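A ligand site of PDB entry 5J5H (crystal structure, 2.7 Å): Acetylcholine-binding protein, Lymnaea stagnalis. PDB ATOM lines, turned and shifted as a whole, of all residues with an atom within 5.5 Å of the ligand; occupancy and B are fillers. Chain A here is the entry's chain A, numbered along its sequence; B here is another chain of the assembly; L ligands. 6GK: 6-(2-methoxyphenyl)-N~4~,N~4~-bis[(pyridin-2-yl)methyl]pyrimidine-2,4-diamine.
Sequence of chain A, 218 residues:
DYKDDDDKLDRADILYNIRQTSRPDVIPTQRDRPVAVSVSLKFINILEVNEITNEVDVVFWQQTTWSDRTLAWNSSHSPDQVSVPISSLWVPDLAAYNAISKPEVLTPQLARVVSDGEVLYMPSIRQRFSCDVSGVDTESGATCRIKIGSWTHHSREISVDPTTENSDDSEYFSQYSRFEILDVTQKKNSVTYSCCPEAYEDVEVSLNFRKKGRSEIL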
ATOM      1  N   TRP A  61      -2.028  29.959 -28.572  1.00  0.00           N
ATOM      2  CA  TRP A  61      -1.978  28.710 -27.825  1.00  0.00           C
ATOM      3  C   TRP A  61      -0.550  28.212 -27.720  1.00  0.00           C
ATOM      4  O   TRP A  61       0.058  27.890 -28.727  1.00  0.00           O
ATOM      5  CB  TRP A  61      -2.817  27.636 -28.520  1.00  0.00           C
ATOM      6  CG  TRP A  61      -4.269  27.808 -28.442  1.00  0.00           C
ATOM      7  CD1 TRP A  61      -4.950  28.853 -27.857  1.00  0.00           C
ATOM      8  CD2 TRP A  61      -5.248  26.906 -28.934  1.00  0.00           C
ATOM      9  NE1 TRP A  61      -6.305  28.649 -27.985  1.00  0.00           N
ATOM     10  CE2 TRP A  61      -6.520  27.460 -28.637  1.00  0.00           C
ATOM     11  CE3 TRP A  61      -5.185  25.689 -29.617  1.00  0.00           C
ATOM     12  CZ2 TRP A  61      -7.705  26.839 -28.999  1.00  0.00           C
ATOM     13  CZ3 TRP A  61      -6.371  25.069 -29.979  1.00  0.00           C
ATOM     14  CH2 TRP A  61      -7.613  25.641 -29.658  1.00  0.00           C
ATOM     15  N   GLN A  63       1.839  25.486 -27.111  1.00  0.00           N
ATOM     16  CA  GLN A  63       2.120  24.068 -26.961  1.00  0.00           C
ATOM     17  C   GLN A  63       3.479  23.885 -26.298  1.00  0.00           C
ATOM     18  O   GLN A  63       4.503  24.189 -26.903  1.00  0.00           O
ATOM     19  CB  GLN A  63       2.096  23.360 -28.302  1.00  0.00           C
ATOM     20  CG  GLN A  63       0.799  23.602 -29.050  1.00  0.00           C
ATOM     21  CD  GLN A  63       0.733  22.891 -30.379  1.00  0.00           C
ATOM     22  OE1 GLN A  63      -0.308  22.364 -30.762  1.00  0.00           O
ATOM     23  NE2 GLN A  63       1.847  22.869 -31.086  1.00  0.00           N
ATOM     24  N   THR A  64       3.457  23.396 -25.056  1.00  0.00           N
ATOM     25  CA  THR A  64       4.671  23.194 -24.288  1.00  0.00           C
ATOM     26  C   THR A  64       4.741  21.741 -23.880  1.00  0.00           C
ATOM     27  O   THR A  64       3.739  21.156 -23.436  1.00  0.00           O
ATOM     28  CB  THR A  64       4.750  24.107 -23.030  1.00  0.00           C
ATOM     29  OG1 THR A  64       4.243  25.416 -23.326  1.00  0.00           O
ATOM     30  CG2 THR A  64       6.186  24.203 -22.536  1.00  0.00           C
ATOM     31  N   THR A  65       5.934  21.155 -24.034  1.00  0.00           N
ATOM     32  CA  THR A  65       6.128  19.756 -23.716  1.00  0.00           C
ATOM     33  C   THR A  65       7.554  19.530 -23.273  1.00  0.00           C
ATOM     34  O   THR A  65       8.476  20.160 -23.768  1.00  0.00           O
ATOM     35  CB  THR A  65       5.795  18.820 -24.924  1.00  0.00           C
ATOM     36  OG1 THR A  65       6.213  17.485 -24.641  1.00  0.00           O
ATOM     37  CG2 THR A  65       6.486  19.280 -26.151  1.00  0.00           C
ATOM     38  N   LEU A 110      -4.378  23.323 -16.309  1.00  0.00           N
ATOM     39  CA  LEU A 110      -4.041  21.894 -16.156  1.00  0.00           C
ATOM     40  C   LEU A 110      -2.995  21.501 -17.191  1.00  0.00           C
ATOM     41  O   LEU A 110      -2.801  22.192 -18.213  1.00  0.00           O
ATOM     42  CB  LEU A 110      -5.288  21.013 -16.290  1.00  0.00           C
ATOM     43  CG  LEU A 110      -6.545  21.515 -15.550  1.00  0.00           C
ATOM     44  CD1 LEU A 110      -7.751  20.700 -15.932  1.00  0.00           C
ATOM     45  CD2 LEU A 110      -6.393  21.475 -14.062  1.00  0.00           C
ATOM     46  N   ALA A 111      -2.285  20.402 -16.906  1.00  0.00           N
ATOM     47  CA  ALA A 111      -1.407  19.764 -17.887  1.00  0.00           C
ATOM     48  C   ALA A 111      -1.826  18.328 -18.019  1.00  0.00           C
ATOM     49  O   ALA A 111      -2.544  17.811 -17.159  1.00  0.00           O
ATOM     50  CB  ALA A 111       0.068  19.845 -17.485  1.00  0.00           C
ATOM     51  N   ARG A 112      -1.378  17.694 -19.106  1.00  0.00           N
ATOM     52  CA  ARG A 112      -1.572  16.262 -19.312  1.00  0.00           C
ATOM     53  C   ARG A 112      -0.278  15.543 -19.030  1.00  0.00           C
ATOM     54  O   ARG A 112       0.724  15.805 -19.674  1.00  0.00           O
ATOM     55  CB  ARG A 112      -2.026  15.975 -20.737  1.00  0.00           C
ATOM     56  CG  ARG A 112      -3.407  16.469 -21.010  1.00  0.00           C
ATOM     57  CD  ARG A 112      -4.407  15.651 -20.234  1.00  0.00           C
ATOM     58  NE  ARG A 112      -4.588  14.346 -20.857  1.00  0.00           N
ATOM     59  CZ  ARG A 112      -5.573  13.520 -20.542  1.00  0.00           C
ATOM     60  NH1 ARG A 112      -6.457  13.889 -19.608  1.00  0.00           N
ATOM     61  NH2 ARG A 112      -5.688  12.355 -21.174  1.00  0.00           N
ATOM     62  N   LEU A 120       2.312  17.466 -21.238  1.00  0.00           N
ATOM     63  CA  LEU A 120       1.777  18.271 -22.322  1.00  0.00           C
ATOM     64  C   LEU A 120       1.035  19.429 -21.710  1.00  0.00           C
ATOM     65  O   LEU A 120       0.055  19.254 -21.003  1.00  0.00           O
ATOM     66  CB  LEU A 120       0.842  17.441 -23.225  1.00  0.00           C
ATOM     67  CG  LEU A 120       1.428  16.224 -23.962  1.00  0.00           C
ATOM     68  CD1 LEU A 120       0.332  15.403 -24.638  1.00  0.00           C
ATOM     69  CD2 LEU A 120       2.415  16.690 -25.004  1.00  0.00           C
ATOM     70  N   TYR A 121       1.527  20.631 -21.967  1.00  0.00           N
ATOM     71  CA  TYR A 121       0.947  21.812 -21.367  1.00  0.00           C
ATOM     72  C   TYR A 121       0.697  22.860 -22.464  1.00  0.00           C
ATOM     73  O   TYR A 121       1.567  23.124 -23.298  1.00  0.00           O
ATOM     74  CB  TYR A 121       1.862  22.336 -20.244  1.00  0.00           C
ATOM     75  CG  TYR A 121       1.367  23.632 -19.647  1.00  0.00           C
ATOM     76  CD1 TYR A 121       0.111  23.705 -19.078  1.00  0.00           C
ATOM     77  CD2 TYR A 121       2.149  24.787 -19.680  1.00  0.00           C
ATOM     78  CE1 TYR A 121      -0.361  24.904 -18.550  1.00  0.00           C
ATOM     79  CE2 TYR A 121       1.692  25.989 -19.137  1.00  0.00           C
ATOM     80  CZ  TYR A 121       0.430  26.024 -18.591  1.00  0.00           C
ATOM     81  OH  TYR A 121      -0.059  27.173 -18.061  1.00  0.00           O
ATOM     82  N   MET A 122      -0.507  23.435 -22.467  1.00  0.00           N
ATOM     83  CA  MET A 122      -0.911  24.317 -23.569  1.00  0.00           C
ATOM     84  C   MET A 122      -1.933  25.380 -23.147  1.00  0.00           C
ATOM     85  O   MET A 122      -3.140  25.242 -23.413  1.00  0.00           O
ATOM     86  CB  MET A 122      -1.469  23.502 -24.730  1.00  0.00           C
ATOM     87  CG  MET A 122      -1.700  24.329 -25.997  1.00  0.00           C
ATOM     88  SD  MET A 122      -2.494  23.439 -27.358  1.00  0.00           S
ATOM     89  CE  MET A 122      -4.214  23.570 -26.949  1.00  0.00           C
ATOM     90  N   TYR A 172      -5.695  26.935 -36.489  1.00  0.00           N
ATOM     91  CA  TYR A 172      -5.944  27.508 -35.198  1.00  0.00           C
ATOM     92  C   TYR A 172      -6.357  28.971 -35.331  1.00  0.00           C
ATOM     93  O   TYR A 172      -7.206  29.460 -34.571  1.00  0.00           O
ATOM     94  CB  TYR A 172      -4.687  27.372 -34.339  1.00  0.00           C
ATOM     95  CG  TYR A 172      -4.180  25.942 -34.214  1.00  0.00           C
ATOM     96  CD1 TYR A 172      -4.711  25.087 -33.255  1.00  0.00           C
ATOM     97  CD2 TYR A 172      -3.197  25.442 -35.067  1.00  0.00           C
ATOM     98  CE1 TYR A 172      -4.266  23.785 -33.138  1.00  0.00           C
ATOM     99  CE2 TYR A 172      -2.749  24.129 -34.958  1.00  0.00           C
ATOM    100  CZ  TYR A 172      -3.289  23.309 -33.990  1.00  0.00           C
ATOM    101  OH  TYR A 172      -2.854  21.996 -33.860  1.00  0.00           O
ATOM    102  N   TYR B  97     -13.047  28.240 -26.638  1.00  0.00           N
ATOM    103  CA  TYR B  97     -11.849  28.133 -27.468  1.00  0.00           C
ATOM    104  C   TYR B  97     -11.567  29.403 -28.255  1.00  0.00           C
ATOM    105  O   TYR B  97     -10.408  29.691 -28.570  1.00  0.00           O
ATOM    106  CB  TYR B  97     -11.961  26.945 -28.428  1.00  0.00           C
ATOM    107  CG  TYR B  97     -12.102  25.580 -27.776  1.00  0.00           C
ATOM    108  CD1 TYR B  97     -11.833  25.370 -26.415  1.00  0.00           C
ATOM    109  CD2 TYR B  97     -12.489  24.483 -28.536  1.00  0.00           C
ATOM    110  CE1 TYR B  97     -11.982  24.105 -25.849  1.00  0.00           C
ATOM    111  CE2 TYR B  97     -12.628  23.229 -27.983  1.00  0.00           C
ATOM    112  CZ  TYR B  97     -12.378  23.029 -26.644  1.00  0.00           C
ATOM    113  OH  TYR B  97     -12.533  21.756 -26.135  1.00  0.00           O
ATOM    114  N   SER B 150     -14.135  20.848 -23.003  1.00  0.00           N
ATOM    115  CA  SER B 150     -13.091  20.475 -22.070  1.00  0.00           C
ATOM    116  C   SER B 150     -11.757  20.913 -22.644  1.00  0.00           C
ATOM    117  O   SER B 150     -11.525  20.798 -23.825  1.00  0.00           O
ATOM    118  CB  SER B 150     -13.101  18.976 -21.811  1.00  0.00           C
ATOM    119  OG  SER B 150     -11.921  18.550 -21.117  1.00  0.00           O
ATOM    120  N   TRP B 151     -10.874  21.402 -21.795  1.00  0.00           N
ATOM    121  CA  TRP B 151      -9.597  21.879 -22.283  1.00  0.00           C
ATOM    122  C   TRP B 151      -8.561  20.782 -22.337  1.00  0.00           C
ATOM    123  O   TRP B 151      -7.594  20.880 -23.079  1.00  0.00           O
ATOM    124  CB  TRP B 151      -9.093  23.050 -21.413  1.00  0.00           C
ATOM    125  CG  TRP B 151      -7.854  23.668 -21.957  1.00  0.00           C
ATOM    126  CD1 TRP B 151      -6.590  23.591 -21.441  1.00  0.00           C
ATOM    127  CD2 TRP B 151      -7.748  24.427 -23.170  1.00  0.00           C
ATOM    128  NE1 TRP B 151      -5.708  24.271 -22.261  1.00  0.00           N
ATOM    129  CE2 TRP B 151      -6.392  24.792 -23.329  1.00  0.00           C
ATOM    130  CE3 TRP B 151      -8.660  24.832 -24.144  1.00  0.00           C
ATOM    131  CZ2 TRP B 151      -5.943  25.551 -24.405  1.00  0.00           C
ATOM    132  CZ3 TRP B 151      -8.199  25.590 -25.212  1.00  0.00           C
ATOM    133  CH2 TRP B 151      -6.871  25.937 -25.331  1.00  0.00           C
ATOM    134  N   THR B 152      -8.717  19.721 -21.544  1.00  0.00           N
ATOM    135  CA  THR B 152      -7.628  18.747 -21.432  1.00  0.00           C
ATOM    136  C   THR B 152      -8.137  17.328 -21.525  1.00  0.00           C
ATOM    137  O   THR B 152      -7.348  16.388 -21.608  1.00  0.00           O
ATOM    138  CB  THR B 152      -6.818  18.882 -20.092  1.00  0.00           C
ATOM    139  OG1 THR B 152      -7.633  18.510 -18.957  1.00  0.00           O
ATOM    140  CG2 THR B 152      -6.256  20.286 -19.927  1.00  0.00           C
ATOM    141  N   VAL B 191     -13.941  17.394 -32.965  1.00  0.00           N
ATOM    142  CA  VAL B 191     -12.803  18.201 -33.352  1.00  0.00           C
ATOM    143  C   VAL B 191     -11.645  17.216 -33.414  1.00  0.00           C
ATOM    144  O   VAL B 191     -11.625  16.225 -32.672  1.00  0.00           O
ATOM    145  CB  VAL B 191     -12.440  19.329 -32.349  1.00  0.00           C
ATOM    146  CG1 VAL B 191     -12.099  18.786 -30.958  1.00  0.00           C
ATOM    147  CG2 VAL B 191     -11.353  20.215 -32.890  1.00  0.00           C
ATOM    148  N   TYR B 193      -7.296  17.501 -34.195  1.00  0.00           N
ATOM    149  CA  TYR B 193      -6.182  18.311 -34.676  1.00  0.00           C
ATOM    150  C   TYR B 193      -5.054  17.484 -35.282  1.00  0.00           C
ATOM    151  O   TYR B 193      -4.691  16.421 -34.762  1.00  0.00           O
ATOM    152  CB  TYR B 193      -5.613  19.186 -33.560  1.00  0.00           C
ATOM    153  CG  TYR B 193      -6.559  20.228 -33.023  1.00  0.00           C
ATOM    154  CD1 TYR B 193      -7.576  19.868 -32.138  1.00  0.00           C
ATOM    155  CD2 TYR B 193      -6.489  21.553 -33.439  1.00  0.00           C
ATOM    156  CE1 TYR B 193      -8.444  20.802 -31.640  1.00  0.00           C
ATOM    157  CE2 TYR B 193      -7.379  22.508 -32.955  1.00  0.00           C
ATOM    158  CZ  TYR B 193      -8.366  22.121 -32.057  1.00  0.00           C
ATOM    159  OH  TYR B 193      -9.260  23.040 -31.561  1.00  0.00           O
ATOM    160  N   CYS B 195      -2.096  17.040 -34.852  1.00  0.00           N
ATOM    161  CA  CYS B 195      -1.195  17.270 -33.729  1.00  0.00           C
ATOM    162  C   CYS B 195      -1.292  16.061 -32.809  1.00  0.00           C
ATOM    163  O   CYS B 195      -0.283  15.439 -32.484  1.00  0.00           O
ATOM    164  CB  CYS B 195      -1.561  18.546 -32.942  1.00  0.00           C
ATOM    165  SG  CYS B 195      -2.744  18.247 -31.572  1.00  0.00           S
ATOM    166  N   CYS B 196      -2.520  15.721 -32.422  1.00  0.00           N
ATOM    167  CA  CYS B 196      -2.789  14.695 -31.419  1.00  0.00           C
ATOM    168  C   CYS B 196      -3.765  13.674 -31.954  1.00  0.00           C
ATOM    169  O   CYS B 196      -4.542  13.975 -32.858  1.00  0.00           O
ATOM    170  CB  CYS B 196      -3.347  15.337 -30.146  1.00  0.00           C
ATOM    171  SG  CYS B 196      -2.777  17.028 -29.946  1.00  0.00           S
ATOM    172  N   TYR B 200     -11.911  15.662 -29.375  1.00  0.00           N
ATOM    173  CA  TYR B 200     -12.360  16.309 -28.139  1.00  0.00           C
ATOM    174  C   TYR B 200     -13.793  16.831 -28.349  1.00  0.00           C
ATOM    175  O   TYR B 200     -14.073  17.549 -29.257  1.00  0.00           O
ATOM    176  CB  TYR B 200     -11.393  17.444 -27.724  1.00  0.00           C
ATOM    177  CG  TYR B 200     -10.038  16.995 -27.151  1.00  0.00           C
ATOM    178  CD1 TYR B 200      -9.178  16.146 -27.857  1.00  0.00           C
ATOM    179  CD2 TYR B 200      -9.601  17.464 -25.899  1.00  0.00           C
ATOM    180  CE1 TYR B 200      -7.939  15.745 -27.328  1.00  0.00           C
ATOM    181  CE2 TYR B 200      -8.356  17.085 -25.362  1.00  0.00           C
ATOM    182  CZ  TYR B 200      -7.543  16.213 -26.078  1.00  0.00           C
ATOM    183  OH  TYR B 200      -6.328  15.831 -25.550  1.00  0.00           O
HETATM  184  C10 6GK L   1      -3.994  19.681 -27.907  1.00  0.00           C
HETATM  185  C13 6GK L   1      -7.090  20.339 -27.598  1.00  0.00           C
HETATM  186  C15 6GK L   1      -9.092  21.679 -27.978  1.00  0.00           C
HETATM  187  C17 6GK L   1      -7.389  22.432 -26.454  1.00  0.00           C
HETATM  188  C20 6GK L   1      -4.621  21.176 -23.499  1.00  0.00           C
HETATM  189  C21 6GK L   1      -3.540  20.741 -22.718  1.00  0.00           C
HETATM  190  C22 6GK L   1      -2.925  19.537 -23.034  1.00  0.00           C
HETATM  191  C01 6GK L   1       1.731  19.632 -30.625  1.00  0.00           C
HETATM  192  O01 6GK L   1       0.498  19.639 -29.881  1.00  0.00           O
HETATM  193  C02 6GK L   1       0.723  19.825 -28.552  1.00  0.00           C
HETATM  194  C07 6GK L   1       2.008  19.773 -28.012  1.00  0.00           C
HETATM  195  C06 6GK L   1       2.231  19.958 -26.655  1.00  0.00           C
HETATM  196  C05 6GK L   1       1.131  20.196 -25.833  1.00  0.00           C
HETATM  197  C04 6GK L   1      -0.163  20.254 -26.359  1.00  0.00           C
HETATM  198  C03 6GK L   1      -0.375  20.052 -27.724  1.00  0.00           C
HETATM  199  C08 6GK L   1      -1.681  20.140 -28.184  1.00  0.00           C
HETATM  200  C11 6GK L   1      -2.703  19.559 -27.442  1.00  0.00           C
HETATM  201  N01 6GK L   1      -1.992  20.823 -29.302  1.00  0.00           N
HETATM  202  C09 6GK L   1      -3.257  20.928 -29.717  1.00  0.00           C
HETATM  203  N02 6GK L   1      -3.550  21.586 -30.828  1.00  0.00           N
HETATM  204  N03 6GK L   1      -4.243  20.359 -29.029  1.00  0.00           N
HETATM  205  N04 6GK L   1      -5.020  19.143 -27.269  1.00  0.00           N
HETATM  206  C18 6GK L   1      -4.878  18.443 -25.969  1.00  0.00           C
HETATM  207  C19 6GK L   1      -4.454  19.240 -24.880  1.00  0.00           C
HETATM  208  N06 6GK L   1      -5.061  20.392 -24.574  1.00  0.00           N
HETATM  209  C23 6GK L   1      -3.381  18.795 -24.114  1.00  0.00           C
HETATM  210  C12 6GK L   1      -6.372  19.164 -27.871  1.00  0.00           C
HETATM  211  N05 6GK L   1      -6.632  21.271 -26.732  1.00  0.00           N
HETATM  212  C16 6GK L   1      -8.615  22.647 -27.080  1.00  0.00           C
HETATM  213  C14 6GK L   1      -8.330  20.538 -28.218  1.00  0.00           C
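The backbone NH (N) of Leu 120 sits at hydrogen-bond distance from the backbone carbonyl oxygen (O) of Arg 112 (2.8 Å).
N of Thr 64 lies within hydrogen-bond range of O of Tyr 121, 2.6 Å away.
O of Ser 150 of chain B is in hydrogen-bond range of OH of Tyr 97 of chain B.
The guanidinium group (NH1) of Arg 112 sits at hydrogen-bond distance from the backbone carbonyl oxygen (O) of Thr 152 of chain B.
NE1 of Trp 151 of chain B lies within hydrogen-bond range of O of Met 122 (3.0 Å).
The backbone NH (N) of Thr 152 of chain B lies within hydrogen-bond range of the side-chain hydroxyl (OG) of Ser 150 of chain B (3.4 Å).
SG of Cys 196 of chain B is disulfide-bonded to SG of Cys 195 of chain B (2.0 Å).
O of Val 191 of chain B sits at hydrogen-bond distance from N of Tyr 200 of chain B (3.4 Å).
N01 of the ligand lies close to OE1 of Gln 63.
The side-chain sulfur (SG) of Cys 195 of chain B lies close to a nitrogen (N02) of the ligand (3.5 Å).
OH of Tyr 172 lies within hydrogen-bond range of N02 of the ligand.
The side-chain sulfur (SD) of Met 122 lies close to a nitrogen (N01) of the ligand.
O of Trp 151 of chain B lies close to N06 of the ligand (3.0 Å).
The side-chain sulfur (SG) of Cys 196 of chain B lies close to a nitrogen (N03) of the ligand (3.8 Å).
Merely in contact with the ligand: Tyr 200 of chain B, Tyr 193 of chain B, Leu 120, Thr 64, Arg 112, Tyr 97 of chain B, Tyr 121 and Thr 152 of chain B.
14 residues have an atom within 4 Å of the ligand: Gln 63, Thr 64, Arg 112, Leu 120, Tyr 121, Met 122, Tyr 172, Tyr 97 of chain B, Trp 151 of chain B, Thr 152 of chain B, Tyr 193 of chain B, Cys 195 of chain B, Cys 196 of chain B and Tyr 200 of chain B.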
